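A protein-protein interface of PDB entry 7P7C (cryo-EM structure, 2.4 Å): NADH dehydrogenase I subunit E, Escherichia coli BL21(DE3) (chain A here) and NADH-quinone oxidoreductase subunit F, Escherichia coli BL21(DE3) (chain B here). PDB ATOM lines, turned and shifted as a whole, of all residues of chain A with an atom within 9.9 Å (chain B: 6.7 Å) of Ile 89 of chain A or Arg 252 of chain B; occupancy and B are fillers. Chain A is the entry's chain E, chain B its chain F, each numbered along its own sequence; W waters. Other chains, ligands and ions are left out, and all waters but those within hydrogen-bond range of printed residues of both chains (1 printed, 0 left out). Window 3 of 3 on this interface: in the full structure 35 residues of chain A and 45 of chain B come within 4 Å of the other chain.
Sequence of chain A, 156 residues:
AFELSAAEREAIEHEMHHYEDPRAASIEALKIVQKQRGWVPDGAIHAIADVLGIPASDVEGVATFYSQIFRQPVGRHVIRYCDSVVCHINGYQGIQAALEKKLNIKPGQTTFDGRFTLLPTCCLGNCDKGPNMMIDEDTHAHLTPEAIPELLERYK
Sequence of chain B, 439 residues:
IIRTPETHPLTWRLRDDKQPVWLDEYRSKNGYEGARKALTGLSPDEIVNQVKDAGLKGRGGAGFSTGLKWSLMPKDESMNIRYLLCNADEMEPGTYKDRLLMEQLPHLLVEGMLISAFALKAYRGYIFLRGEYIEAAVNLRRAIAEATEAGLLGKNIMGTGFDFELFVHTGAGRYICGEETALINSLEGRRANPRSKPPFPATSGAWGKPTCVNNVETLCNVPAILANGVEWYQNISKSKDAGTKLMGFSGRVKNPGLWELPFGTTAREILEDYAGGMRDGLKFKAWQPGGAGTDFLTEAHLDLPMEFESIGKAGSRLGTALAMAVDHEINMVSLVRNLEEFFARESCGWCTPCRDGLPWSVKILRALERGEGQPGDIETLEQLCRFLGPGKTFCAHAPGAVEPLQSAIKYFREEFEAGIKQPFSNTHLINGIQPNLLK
Of the 19 printed residues of chain B, 8 touch a printed residue of chain A.
Hydrophobic or aromatic side chains of chain B within 4 Å of the printed part of chain A: Pro 256, Met 324, Val 326 and Leu 335.
Of the 20 printed residues of chain A, 6 touch a printed residue of chain B.
Among the printed residues, 12 pairs touch across the chains.
Val 85 of chain A touches Met 324 of chain B (CG2 to SD, 3.7 Å).
Val 85 of chain A touches Leu 335 of chain B.
Val 86 of chain A touches Ser 250 of chain B (CG1 to OG, 3.7 Å).
Val 86 of chain A touches Met 324 of chain B.
CD1 of Leu 335 of chain B touches CD2 of His 88 of chain A, 3.6 Å away.
Ile 89 of chain A touches Met 324 of chain B.
Ala 325 of chain B touches Ile 89 of chain A (O to CD1, 3.7 Å).
Val 326 of chain B touches Ile 89 of chain A (CG2 to CD1, 3.8 Å).
Ile 89 of chain A touches Leu 335 of chain B.
Asp 128 of chain A touches Pro 256 of chain B.
Water W1 lies within hydrogen-bond range of O of Cys 127 of chain A (2.8 Å), N of Gly 251 of chain B (3.0 Å) and ND2 of Asn 90 of chain A (3.1 Å).
OE1 of Gln 93 of chain A is in hydrogen-bond range of ND1 of His 88 of chain A (3.4 Å).
The guanidinium group (NH2) of Arg 252 of chain B lies within salt-bridge range of the side-chain carboxylate (OE1) of Glu 329 of chain B (3.2 Å).
OD2 of Asp 128 of chain A is in salt-bridge range of NZ of Lys 129 of chain A (3.4 Å).
The backbone carbonyl oxygen of Val 86 of chain A is in hydrogen-bond range of the side-chain amide nitrogen of Asn 90 of chain A (3.2 Å).
The backbone NH (N) of Ala 325 of chain B is in hydrogen-bond range of the backbone carbonyl oxygen (O) of Ser 250 of chain B (2.9 Å).
The backbone NH of Arg 279 of chain B is in hydrogen-bond range of the backbone carbonyl oxygen of Arg 252 of chain B (3.1 Å).
Ile 89 of chain A touches five residues of chain B.
Of chain A, only Ile 89 comes within 4 Å of Arg 252 of chain B.
Gly 251 of chain B touches just one residue of chain A: Asn 90.
Ala 325 of chain B touches just one residue of chain A: Ile 89.
Printed residues of chain B within 4 Å of His 88 of chain A: Leu 335 (3.6 Å).
Printed residues of chain A within 4 Å of Ser 250 of chain B: Val 86 (3.7 Å).
Of the printed residues of chain B, Val 85 of chain A touches Met 324 (3.7 Å) and Leu 335 (3.7 Å).
Of the printed residues of chain B, Asn 90 of chain A touches Gly 251 (3.5 Å).
Of the printed residues of chain A, Met 324 of chain B touches Val 85, Val 86 and Ile 89.
Cys 82 of chain A touches none of the printed residues of chain B.
The nearest residue of chain B that does not touch Ile 89 of chain A is Asp 327 of chain B (4.2 Å).
The guanidinium group of Arg 252 of chain B is in hydrogen-bond range of the backbone carbonyl oxygen of Ile 89 of chain A (3.1 Å).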
ATOM      1  N   CYS A  82      -7.262 -16.667  -7.340  1.00  0.00           N
ATOM      2  CA  CYS A  82      -6.232 -15.717  -7.724  1.00  0.00           C
ATOM      3  C   CYS A  82      -5.019 -16.455  -8.272  1.00  0.00           C
ATOM      4  O   CYS A  82      -4.473 -17.342  -7.611  1.00  0.00           O
ATOM      5  CB  CYS A  82      -5.833 -14.856  -6.529  1.00  0.00           C
ATOM      6  SG  CYS A  82      -4.513 -13.694  -6.878  1.00  0.00           S
ATOM      7  N   ASP A  83      -4.593 -16.088  -9.482  1.00  0.00           N
ATOM      8  CA  ASP A  83      -3.408 -16.679 -10.089  1.00  0.00           C
ATOM      9  C   ASP A  83      -2.279 -15.667 -10.239  1.00  0.00           C
ATOM     10  O   ASP A  83      -1.388 -15.855 -11.072  1.00  0.00           O
ATOM     11  CB  ASP A  83      -3.746 -17.314 -11.444  1.00  0.00           C
ATOM     12  CG  ASP A  83      -4.112 -16.301 -12.507  1.00  0.00           C
ATOM     13  OD1 ASP A  83      -4.767 -15.298 -12.193  1.00  0.00           O
ATOM     14  OD2 ASP A  83      -3.745 -16.525 -13.677  1.00  0.00           O
ATOM     15  N   SER A  84      -2.291 -14.606  -9.438  1.00  0.00           N
ATOM     16  CA  SER A  84      -1.300 -13.546  -9.554  1.00  0.00           C
ATOM     17  C   SER A  84      -0.036 -13.925  -8.784  1.00  0.00           C
ATOM     18  O   SER A  84       0.099 -15.037  -8.270  1.00  0.00           O
ATOM     19  CB  SER A  84      -1.889 -12.219  -9.088  1.00  0.00           C
ATOM     20  OG  SER A  84      -2.692 -11.644 -10.101  1.00  0.00           O
ATOM     21  N   VAL A  85       0.899 -12.978  -8.688  1.00  0.00           N
ATOM     22  CA  VAL A  85       2.286 -13.306  -8.367  1.00  0.00           C
ATOM     23  C   VAL A  85       2.452 -13.694  -6.897  1.00  0.00           C
ATOM     24  O   VAL A  85       3.156 -14.661  -6.579  1.00  0.00           O
ATOM     25  CB  VAL A  85       3.203 -12.137  -8.781  1.00  0.00           C
ATOM     26  CG1 VAL A  85       2.708 -10.799  -8.231  1.00  0.00           C
ATOM     27  CG2 VAL A  85       4.637 -12.398  -8.384  1.00  0.00           C
ATOM     28  N   VAL A  86       1.814 -12.964  -5.979  1.00  0.00           N
ATOM     29  CA  VAL A  86       1.996 -13.249  -4.558  1.00  0.00           C
ATOM     30  C   VAL A  86       1.325 -14.563  -4.186  1.00  0.00           C
ATOM     31  O   VAL A  86       1.862 -15.346  -3.394  1.00  0.00           O
ATOM     32  CB  VAL A  86       1.480 -12.084  -3.696  1.00  0.00           C
ATOM     33  CG1 VAL A  86       2.012 -12.204  -2.280  1.00  0.00           C
ATOM     34  CG2 VAL A  86       1.877 -10.751  -4.307  1.00  0.00           C
ATOM     35  N   CYS A  87       0.150 -14.831  -4.753  1.00  0.00           N
ATOM     36  CA  CYS A  87      -0.495 -16.116  -4.522  1.00  0.00           C
ATOM     37  C   CYS A  87       0.234 -17.245  -5.242  1.00  0.00           C
ATOM     38  O   CYS A  87       0.134 -18.403  -4.828  1.00  0.00           O
ATOM     39  CB  CYS A  87      -1.958 -16.045  -4.950  1.00  0.00           C
ATOM     40  SG  CYS A  87      -2.957 -14.968  -3.900  1.00  0.00           S
ATOM     41  N   HIS A  88       0.959 -16.929  -6.319  1.00  0.00           N
ATOM     42  CA  HIS A  88       1.857 -17.909  -6.923  1.00  0.00           C
ATOM     43  C   HIS A  88       2.994 -18.262  -5.977  1.00  0.00           C
ATOM     44  O   HIS A  88       3.385 -19.431  -5.875  1.00  0.00           O
ATOM     45  CB  HIS A  88       2.406 -17.375  -8.247  1.00  0.00           C
ATOM     46  CG  HIS A  88       3.479 -18.228  -8.850  1.00  0.00           C
ATOM     47  ND1 HIS A  88       3.208 -19.244  -9.740  1.00  0.00           N
ATOM     48  CD2 HIS A  88       4.824 -18.208  -8.702  1.00  0.00           C
ATOM     49  CE1 HIS A  88       4.339 -19.818 -10.109  1.00  0.00           C
ATOM     50  NE2 HIS A  88       5.335 -19.209  -9.492  1.00  0.00           N
ATOM     51  N   ILE A  89       3.547 -17.259  -5.291  1.00  0.00           N
ATOM     52  CA  ILE A  89       4.572 -17.514  -4.285  1.00  0.00           C
ATOM     53  C   ILE A  89       3.986 -18.299  -3.117  1.00  0.00           C
ATOM     54  O   ILE A  89       4.603 -19.241  -2.608  1.00  0.00           O
ATOM     55  CB  ILE A  89       5.205 -16.185  -3.831  1.00  0.00           C
ATOM     56  CG1 ILE A  89       5.983 -15.559  -4.985  1.00  0.00           C
ATOM     57  CG2 ILE A  89       6.125 -16.393  -2.651  1.00  0.00           C
ATOM     58  CD1 ILE A  89       6.648 -14.254  -4.641  1.00  0.00           C
ATOM     59  N   ASN A  90       2.769 -17.949  -2.702  1.00  0.00           N
ATOM     60  CA  ASN A  90       2.108 -18.635  -1.600  1.00  0.00           C
ATOM     61  C   ASN A  90       1.526 -19.985  -1.996  1.00  0.00           C
ATOM     62  O   ASN A  90       1.009 -20.694  -1.128  1.00  0.00           O
ATOM     63  CB  ASN A  90       1.006 -17.751  -1.019  1.00  0.00           C
ATOM     64  CG  ASN A  90       1.555 -16.567  -0.260  1.00  0.00           C
ATOM     65  OD1 ASN A  90       2.562 -16.676   0.436  1.00  0.00           O
ATOM     66  ND2 ASN A  90       0.898 -15.425  -0.391  1.00  0.00           N
ATOM     67  N   GLY A  91       1.583 -20.352  -3.273  1.00  0.00           N
ATOM     68  CA  GLY A  91       1.185 -21.681  -3.690  1.00  0.00           C
ATOM     69  C   GLY A  91      -0.249 -21.817  -4.152  1.00  0.00           C
ATOM     70  O   GLY A  91      -0.984 -22.666  -3.642  1.00  0.00           O
ATOM     71  N   TYR A  92      -0.668 -20.994  -5.117  1.00  0.00           N
ATOM     72  CA  TYR A  92      -2.008 -21.150  -5.669  1.00  0.00           C
ATOM     73  C   TYR A  92      -2.127 -22.384  -6.549  1.00  0.00           C
ATOM     74  O   TYR A  92      -3.248 -22.826  -6.810  1.00  0.00           O
ATOM     75  CB  TYR A  92      -2.425 -19.899  -6.462  1.00  0.00           C
ATOM     76  CG  TYR A  92      -2.128 -19.936  -7.955  1.00  0.00           C
ATOM     77  CD1 TYR A  92      -0.910 -19.497  -8.444  1.00  0.00           C
ATOM     78  CD2 TYR A  92      -3.080 -20.375  -8.875  1.00  0.00           C
ATOM     79  CE1 TYR A  92      -0.630 -19.520  -9.794  1.00  0.00           C
ATOM     80  CE2 TYR A  92      -2.801 -20.422 -10.220  1.00  0.00           C
ATOM     81  CZ  TYR A  92      -1.578 -19.980 -10.676  1.00  0.00           C
ATOM     82  OH  TYR A  92      -1.302 -20.003 -12.022  1.00  0.00           O
ATOM     83  N   GLN A  93      -1.008 -22.923  -7.044  1.00  0.00           N
ATOM     84  CA  GLN A  93      -1.081 -24.052  -7.969  1.00  0.00           C
ATOM     85  C   GLN A  93      -1.595 -25.312  -7.286  1.00  0.00           C
ATOM     86  O   GLN A  93      -2.307 -26.102  -7.914  1.00  0.00           O
ATOM     87  CB  GLN A  93       0.282 -24.304  -8.612  1.00  0.00           C
ATOM     88  CG  GLN A  93       0.520 -23.481  -9.869  1.00  0.00           C
ATOM     89  CD  GLN A  93       1.893 -22.846  -9.912  1.00  0.00           C
ATOM     90  OE1 GLN A  93       2.430 -22.427  -8.890  1.00  0.00           O
ATOM     91  NE2 GLN A  93       2.468 -22.766 -11.106  1.00  0.00           N
ATOM     92  N   GLY A  94      -1.268 -25.507  -6.008  1.00  0.00           N
ATOM     93  CA  GLY A  94      -1.874 -26.597  -5.261  1.00  0.00           C
ATOM     94  C   GLY A  94      -3.371 -26.422  -5.096  1.00  0.00           C
ATOM     95  O   GLY A  94      -4.129 -27.393  -5.161  1.00  0.00           O
ATOM     96  N   ILE A  95      -3.817 -25.179  -4.899  1.00  0.00           N
ATOM     97  CA  ILE A  95      -5.245 -24.888  -4.804  1.00  0.00           C
ATOM     98  C   ILE A  95      -5.940 -25.173  -6.128  1.00  0.00           C
ATOM     99  O   ILE A  95      -7.040 -25.738  -6.160  1.00  0.00           O
ATOM    100  CB  ILE A  95      -5.462 -23.431  -4.358  1.00  0.00           C
ATOM    101  CG1 ILE A  95      -4.592 -23.113  -3.144  1.00  0.00           C
ATOM    102  CG2 ILE A  95      -6.926 -23.173  -4.052  1.00  0.00           C
ATOM    103  CD1 ILE A  95      -4.913 -23.950  -1.940  1.00  0.00           C
ATOM    104  N   CYS A 127      -3.175 -10.018  -0.596  1.00  0.00           N
ATOM    105  CA  CYS A 127      -1.950 -10.765  -0.855  1.00  0.00           C
ATOM    106  C   CYS A 127      -1.230 -11.164   0.424  1.00  0.00           C
ATOM    107  O   CYS A 127      -0.486 -12.150   0.428  1.00  0.00           O
ATOM    108  CB  CYS A 127      -1.030  -9.940  -1.748  1.00  0.00           C
ATOM    109  SG  CYS A 127      -1.931  -8.964  -2.952  1.00  0.00           S
ATOM    110  N   ASP A 128      -1.430 -10.424   1.515  1.00  0.00           N
ATOM    111  CA  ASP A 128      -0.816 -10.801   2.780  1.00  0.00           C
ATOM    112  C   ASP A 128      -1.483 -12.012   3.418  1.00  0.00           C
ATOM    113  O   ASP A 128      -0.917 -12.587   4.353  1.00  0.00           O
ATOM    114  CB  ASP A 128      -0.841  -9.622   3.753  1.00  0.00           C
ATOM    115  CG  ASP A 128      -2.178  -8.909   3.773  1.00  0.00           C
ATOM    116  OD1 ASP A 128      -3.008  -9.166   2.879  1.00  0.00           O
ATOM    117  OD2 ASP A 128      -2.395  -8.086   4.686  1.00  0.00           O
ATOM    118  N   LYS A 129      -2.661 -12.411   2.940  1.00  0.00           N
ATOM    119  CA  LYS A 129      -3.392 -13.554   3.470  1.00  0.00           C
ATOM    120  C   LYS A 129      -3.548 -14.648   2.420  1.00  0.00           C
ATOM    121  O   LYS A 129      -4.470 -15.460   2.493  1.00  0.00           O
ATOM    122  CB  LYS A 129      -4.758 -13.115   3.992  1.00  0.00           C
ATOM    123  CG  LYS A 129      -4.705 -11.948   4.957  1.00  0.00           C
ATOM    124  CD  LYS A 129      -6.095 -11.423   5.259  1.00  0.00           C
ATOM    125  CE  LYS A 129      -6.061 -10.372   6.355  1.00  0.00           C
ATOM    126  NZ  LYS A 129      -5.320  -9.155   5.933  1.00  0.00           N
ATOM    127  N   GLY A 130      -2.649 -14.683   1.442  1.00  0.00           N
ATOM    128  CA  GLY A 130      -2.760 -15.600   0.333  1.00  0.00           C
ATOM    129  C   GLY A 130      -2.442 -17.037   0.697  1.00  0.00           C
ATOM    130  O   GLY A 130      -1.875 -17.318   1.757  1.00  0.00           O
ATOM    131  N   PRO A 131      -2.804 -17.989  -0.182  1.00  0.00           N
ATOM    132  CA  PRO A 131      -3.540 -17.790  -1.438  1.00  0.00           C
ATOM    133  C   PRO A 131      -5.035 -17.573  -1.224  1.00  0.00           C
ATOM    134  O   PRO A 131      -5.616 -18.121  -0.291  1.00  0.00           O
ATOM    135  CB  PRO A 131      -3.281 -19.089  -2.202  1.00  0.00           C
ATOM    136  CG  PRO A 131      -3.044 -20.096  -1.154  1.00  0.00           C
ATOM    137  CD  PRO A 131      -2.376 -19.387  -0.016  1.00  0.00           C
ATOM    138  N   ASN A 132      -5.642 -16.767  -2.088  1.00  0.00           N
ATOM    139  CA  ASN A 132      -7.020 -16.338  -1.928  1.00  0.00           C
ATOM    140  C   ASN A 132      -7.864 -16.843  -3.085  1.00  0.00           C
ATOM    141  O   ASN A 132      -7.357 -17.090  -4.181  1.00  0.00           O
ATOM    142  CB  ASN A 132      -7.124 -14.811  -1.870  1.00  0.00           C
ATOM    143  CG  ASN A 132      -6.165 -14.203  -0.885  1.00  0.00           C
ATOM    144  OD1 ASN A 132      -6.357 -14.303   0.321  1.00  0.00           O
ATOM    145  ND2 ASN A 132      -5.117 -13.570  -1.393  1.00  0.00           N
ATOM    146  N   SER B 250       4.961  -8.707   1.743  1.00  0.00           N
ATOM    147  CA  SER B 250       4.195  -9.918   1.507  1.00  0.00           C
ATOM    148  C   SER B 250       5.124 -11.004   0.983  1.00  0.00           C
ATOM    149  O   SER B 250       6.296 -10.763   0.686  1.00  0.00           O
ATOM    150  CB  SER B 250       3.047  -9.666   0.523  1.00  0.00           C
ATOM    151  OG  SER B 250       3.536  -9.218  -0.727  1.00  0.00           O
ATOM    152  N   GLY B 251       4.586 -12.217   0.875  1.00  0.00           N
ATOM    153  CA  GLY B 251       5.351 -13.366   0.442  1.00  0.00           C
ATOM    154  C   GLY B 251       5.452 -14.409   1.540  1.00  0.00           C
ATOM    155  O   GLY B 251       4.563 -14.527   2.392  1.00  0.00           O
ATOM    156  N   ARG B 252       6.549 -15.161   1.514  1.00  0.00           N
ATOM    157  CA  ARG B 252       6.793 -16.196   2.517  1.00  0.00           C
ATOM    158  C   ARG B 252       7.591 -15.624   3.689  1.00  0.00           C
ATOM    159  O   ARG B 252       8.669 -16.093   4.047  1.00  0.00           O
ATOM    160  CB  ARG B 252       7.501 -17.388   1.887  1.00  0.00           C
ATOM    161  CG  ARG B 252       6.851 -17.891   0.615  1.00  0.00           C
ATOM    162  CD  ARG B 252       6.231 -19.263   0.803  1.00  0.00           C
ATOM    163  NE  ARG B 252       7.227 -20.324   0.726  1.00  0.00           N
ATOM    164  CZ  ARG B 252       7.676 -20.853  -0.403  1.00  0.00           C
ATOM    165  NH1 ARG B 252       7.232 -20.449  -1.581  1.00  0.00           N
ATOM    166  NH2 ARG B 252       8.595 -21.814  -0.349  1.00  0.00           N
ATOM    167  N   VAL B 253       7.031 -14.578   4.282  1.00  0.00           N
ATOM    168  CA  VAL B 253       7.597 -13.959   5.458  1.00  0.00           C
ATOM    169  C   VAL B 253       6.797 -14.410   6.674  1.00  0.00           C
ATOM    170  O   VAL B 253       5.706 -14.960   6.557  1.00  0.00           O
ATOM    171  CB  VAL B 253       7.628 -12.419   5.337  1.00  0.00           C
ATOM    172  CG1 VAL B 253       8.630 -11.997   4.284  1.00  0.00           C
ATOM    173  CG2 VAL B 253       6.251 -11.890   4.998  1.00  0.00           C
ATOM    174  N   LYS B 254       7.357 -14.185   7.864  1.00  0.00           N
ATOM    175  CA  LYS B 254       6.717 -14.671   9.082  1.00  0.00           C
ATOM    176  C   LYS B 254       5.448 -13.891   9.400  1.00  0.00           C
ATOM    177  O   LYS B 254       4.447 -14.476   9.832  1.00  0.00           O
ATOM    178  CB  LYS B 254       7.696 -14.601  10.253  1.00  0.00           C
ATOM    179  CG  LYS B 254       8.745 -15.697  10.246  1.00  0.00           C
ATOM    180  CD  LYS B 254       9.564 -15.674  11.522  1.00  0.00           C
ATOM    181  CE  LYS B 254      10.745 -16.623  11.442  1.00  0.00           C
ATOM    182  NZ  LYS B 254      10.323 -18.044  11.539  1.00  0.00           N
ATOM    183  N   ASN B 255       5.462 -12.576   9.193  1.00  0.00           N
ATOM    184  CA  ASN B 255       4.318 -11.715   9.483  1.00  0.00           C
ATOM    185  C   ASN B 255       4.028 -10.825   8.282  1.00  0.00           C
ATOM    186  O   ASN B 255       4.415  -9.650   8.257  1.00  0.00           O
ATOM    187  CB  ASN B 255       4.570 -10.873  10.734  1.00  0.00           C
ATOM    188  CG  ASN B 255       3.343 -10.108  11.177  1.00  0.00           C
ATOM    189  OD1 ASN B 255       2.213 -10.515  10.907  1.00  0.00           O
ATOM    190  ND2 ASN B 255       3.557  -8.989  11.854  1.00  0.00           N
ATOM    191  N   PRO B 256       3.343 -11.346   7.264  1.00  0.00           N
ATOM    192  CA  PRO B 256       2.952 -10.492   6.137  1.00  0.00           C
ATOM    193  C   PRO B 256       1.831  -9.549   6.549  1.00  0.00           C
ATOM    194  O   PRO B 256       0.823  -9.972   7.117  1.00  0.00           O
ATOM    195  CB  PRO B 256       2.496 -11.491   5.070  1.00  0.00           C
ATOM    196  CG  PRO B 256       2.086 -12.694   5.827  1.00  0.00           C
ATOM    197  CD  PRO B 256       2.887 -12.737   7.094  1.00  0.00           C
ATOM    198  N   GLY B 277      11.022 -11.106   9.138  1.00  0.00           N
ATOM    199  CA  GLY B 277      11.963 -11.846   8.330  1.00  0.00           C
ATOM    200  C   GLY B 277      11.287 -12.951   7.544  1.00  0.00           C
ATOM    201  O   GLY B 277      10.064 -13.110   7.546  1.00  0.00           O
ATOM    202  N   MET B 278      12.115 -13.734   6.859  1.00  0.00           N
ATOM    203  CA  MET B 278      11.606 -14.855   6.087  1.00  0.00           C
ATOM    204  C   MET B 278      11.200 -15.995   7.018  1.00  0.00           C
ATOM    205  O   MET B 278      11.499 -16.000   8.214  1.00  0.00           O
ATOM    206  CB  MET B 278      12.652 -15.337   5.084  1.00  0.00           C
ATOM    207  CG  MET B 278      13.153 -14.261   4.138  1.00  0.00           C
ATOM    208  SD  MET B 278      11.883 -13.669   3.005  1.00  0.00           S
ATOM    209  CE  MET B 278      11.523 -15.162   2.089  1.00  0.00           C
ATOM    210  N   ARG B 279      10.503 -16.976   6.449  1.00  0.00           N
ATOM    211  CA  ARG B 279      10.135 -18.160   7.205  1.00  0.00           C
ATOM    212  C   ARG B 279      11.365 -19.028   7.467  1.00  0.00           C
ATOM    213  O   ARG B 279      12.447 -18.812   6.915  1.00  0.00           O
ATOM    214  CB  ARG B 279       9.079 -18.972   6.461  1.00  0.00           C
ATOM    215  CG  ARG B 279       7.675 -18.418   6.548  1.00  0.00           C
ATOM    216  CD  ARG B 279       6.724 -19.311   5.779  1.00  0.00           C
ATOM    217  NE  ARG B 279       5.418 -18.696   5.586  1.00  0.00           N
ATOM    218  CZ  ARG B 279       4.501 -19.150   4.744  1.00  0.00           C
ATOM    219  NH1 ARG B 279       4.717 -20.221   4.000  1.00  0.00           N
ATOM    220  NH2 ARG B 279       3.339 -18.512   4.644  1.00  0.00           N
ATOM    221  N   ASP B 280      11.184 -20.024   8.328  1.00  0.00           N
ATOM    222  CA  ASP B 280      12.273 -20.928   8.669  1.00  0.00           C
ATOM    223  C   ASP B 280      12.621 -21.810   7.477  1.00  0.00           C
ATOM    224  O   ASP B 280      11.736 -22.377   6.829  1.00  0.00           O
ATOM    225  CB  ASP B 280      11.891 -21.787   9.871  1.00  0.00           C
ATOM    226  CG  ASP B 280      11.941 -21.017  11.176  1.00  0.00           C
ATOM    227  OD1 ASP B 280      12.787 -20.105  11.295  1.00  0.00           O
ATOM    228  OD2 ASP B 280      11.135 -21.320  12.080  1.00  0.00           O
ATOM    229  N   LEU B 282      14.028 -20.771   4.649  1.00  0.00           N
ATOM    230  CA  LEU B 282      13.887 -20.061   3.385  1.00  0.00           C
ATOM    231  C   LEU B 282      14.926 -18.954   3.316  1.00  0.00           C
ATOM    232  O   LEU B 282      15.071 -18.172   4.261  1.00  0.00           O
ATOM    233  CB  LEU B 282      12.478 -19.483   3.227  1.00  0.00           C
ATOM    234  CG  LEU B 282      11.370 -20.527   3.084  1.00  0.00           C
ATOM    235  CD1 LEU B 282      10.021 -19.861   2.940  1.00  0.00           C
ATOM    236  CD2 LEU B 282      11.645 -21.433   1.901  1.00  0.00           C
ATOM    237  N   MET B 324       7.240  -7.223  -1.940  1.00  0.00           N
ATOM    238  CA  MET B 324       7.000  -8.657  -1.990  1.00  0.00           C
ATOM    239  C   MET B 324       8.342  -9.370  -2.014  1.00  0.00           C
ATOM    240  O   MET B 324       9.205  -9.039  -2.830  1.00  0.00           O
ATOM    241  CB  MET B 324       6.168  -9.029  -3.220  1.00  0.00           C
ATOM    242  CG  MET B 324       6.117 -10.506  -3.521  1.00  0.00           C
ATOM    243  SD  MET B 324       5.515 -10.809  -5.190  1.00  0.00           S
ATOM    244  CE  MET B 324       7.055 -10.760  -6.099  1.00  0.00           C
ATOM    245  N   ALA B 325       8.516 -10.340  -1.123  1.00  0.00           N
ATOM    246  CA  ALA B 325       9.768 -11.070  -0.992  1.00  0.00           C
ATOM    247  C   ALA B 325       9.704 -12.371  -1.779  1.00  0.00           C
ATOM    248  O   ALA B 325       8.668 -13.039  -1.812  1.00  0.00           O
ATOM    249  CB  ALA B 325      10.080 -11.363   0.474  1.00  0.00           C
ATOM    250  N   VAL B 326      10.818 -12.721  -2.412  1.00  0.00           N
ATOM    251  CA  VAL B 326      10.956 -13.938  -3.198  1.00  0.00           C
ATOM    252  C   VAL B 326      12.084 -14.747  -2.582  1.00  0.00           C
ATOM    253  O   VAL B 326      13.225 -14.271  -2.511  1.00  0.00           O
ATOM    254  CB  VAL B 326      11.253 -13.628  -4.673  1.00  0.00           C
ATOM    255  CG1 VAL B 326      11.521 -14.904  -5.441  1.00  0.00           C
ATOM    256  CG2 VAL B 326      10.112 -12.848  -5.293  1.00  0.00           C
ATOM    257  N   ASP B 327      11.770 -15.965  -2.149  1.00  0.00           N
ATOM    258  CA  ASP B 327      12.742 -16.846  -1.527  1.00  0.00           C
ATOM    259  C   ASP B 327      13.514 -17.622  -2.590  1.00  0.00           C
ATOM    260  O   ASP B 327      13.283 -17.485  -3.793  1.00  0.00           O
ATOM    261  CB  ASP B 327      12.054 -17.798  -0.550  1.00  0.00           C
ATOM    262  CG  ASP B 327      10.777 -18.381  -1.109  1.00  0.00           C
ATOM    263  OD1 ASP B 327       9.994 -17.627  -1.720  1.00  0.00           O
ATOM    264  OD2 ASP B 327      10.560 -19.599  -0.948  1.00  0.00           O
ATOM    265  N   GLU B 329      13.452 -20.785  -3.243  1.00  0.00           N
ATOM    266  CA  GLU B 329      12.735 -21.905  -3.836  1.00  0.00           C
ATOM    267  C   GLU B 329      11.855 -21.498  -5.009  1.00  0.00           C
ATOM    268  O   GLU B 329      11.219 -22.367  -5.612  1.00  0.00           O
ATOM    269  CB  GLU B 329      11.880 -22.603  -2.776  1.00  0.00           C
ATOM    270  CG  GLU B 329      12.666 -23.080  -1.569  1.00  0.00           C
ATOM    271  CD  GLU B 329      11.850 -23.975  -0.659  1.00  0.00           C
ATOM    272  OE1 GLU B 329      10.643 -24.156  -0.928  1.00  0.00           O
ATOM    273  OE2 GLU B 329      12.415 -24.498   0.324  1.00  0.00           O
ATOM    274  N   ILE B 330      11.800 -20.217  -5.347  1.00  0.00           N
ATOM    275  CA  ILE B 330      10.966 -19.726  -6.436  1.00  0.00           C
ATOM    276  C   ILE B 330      11.835 -19.588  -7.677  1.00  0.00           C
ATOM    277  O   ILE B 330      12.834 -18.861  -7.669  1.00  0.00           O
ATOM    278  CB  ILE B 330      10.301 -18.389  -6.075  1.00  0.00           C
ATOM    279  CG1 ILE B 330       9.385 -18.557  -4.863  1.00  0.00           C
ATOM    280  CG2 ILE B 330       9.525 -17.844  -7.262  1.00  0.00           C
ATOM    281  CD1 ILE B 330       8.244 -19.517  -5.090  1.00  0.00           C
ATOM    282  N   LEU B 335       8.204 -17.192 -12.154  1.00  0.00           N
ATOM    283  CA  LEU B 335       7.616 -15.998 -11.556  1.00  0.00           C
ATOM    284  C   LEU B 335       7.405 -14.903 -12.592  1.00  0.00           C
ATOM    285  O   LEU B 335       6.338 -14.276 -12.643  1.00  0.00           O
ATOM    286  CB  LEU B 335       8.510 -15.494 -10.428  1.00  0.00           C
ATOM    287  CG  LEU B 335       7.846 -14.514  -9.471  1.00  0.00           C
ATOM    288  CD1 LEU B 335       6.941 -15.273  -8.533  1.00  0.00           C
ATOM    289  CD2 LEU B 335       8.894 -13.744  -8.705  1.00  0.00           C
HETATM  290  O   HOH W   1       1.851 -13.211   1.501  1.00  0.00           O
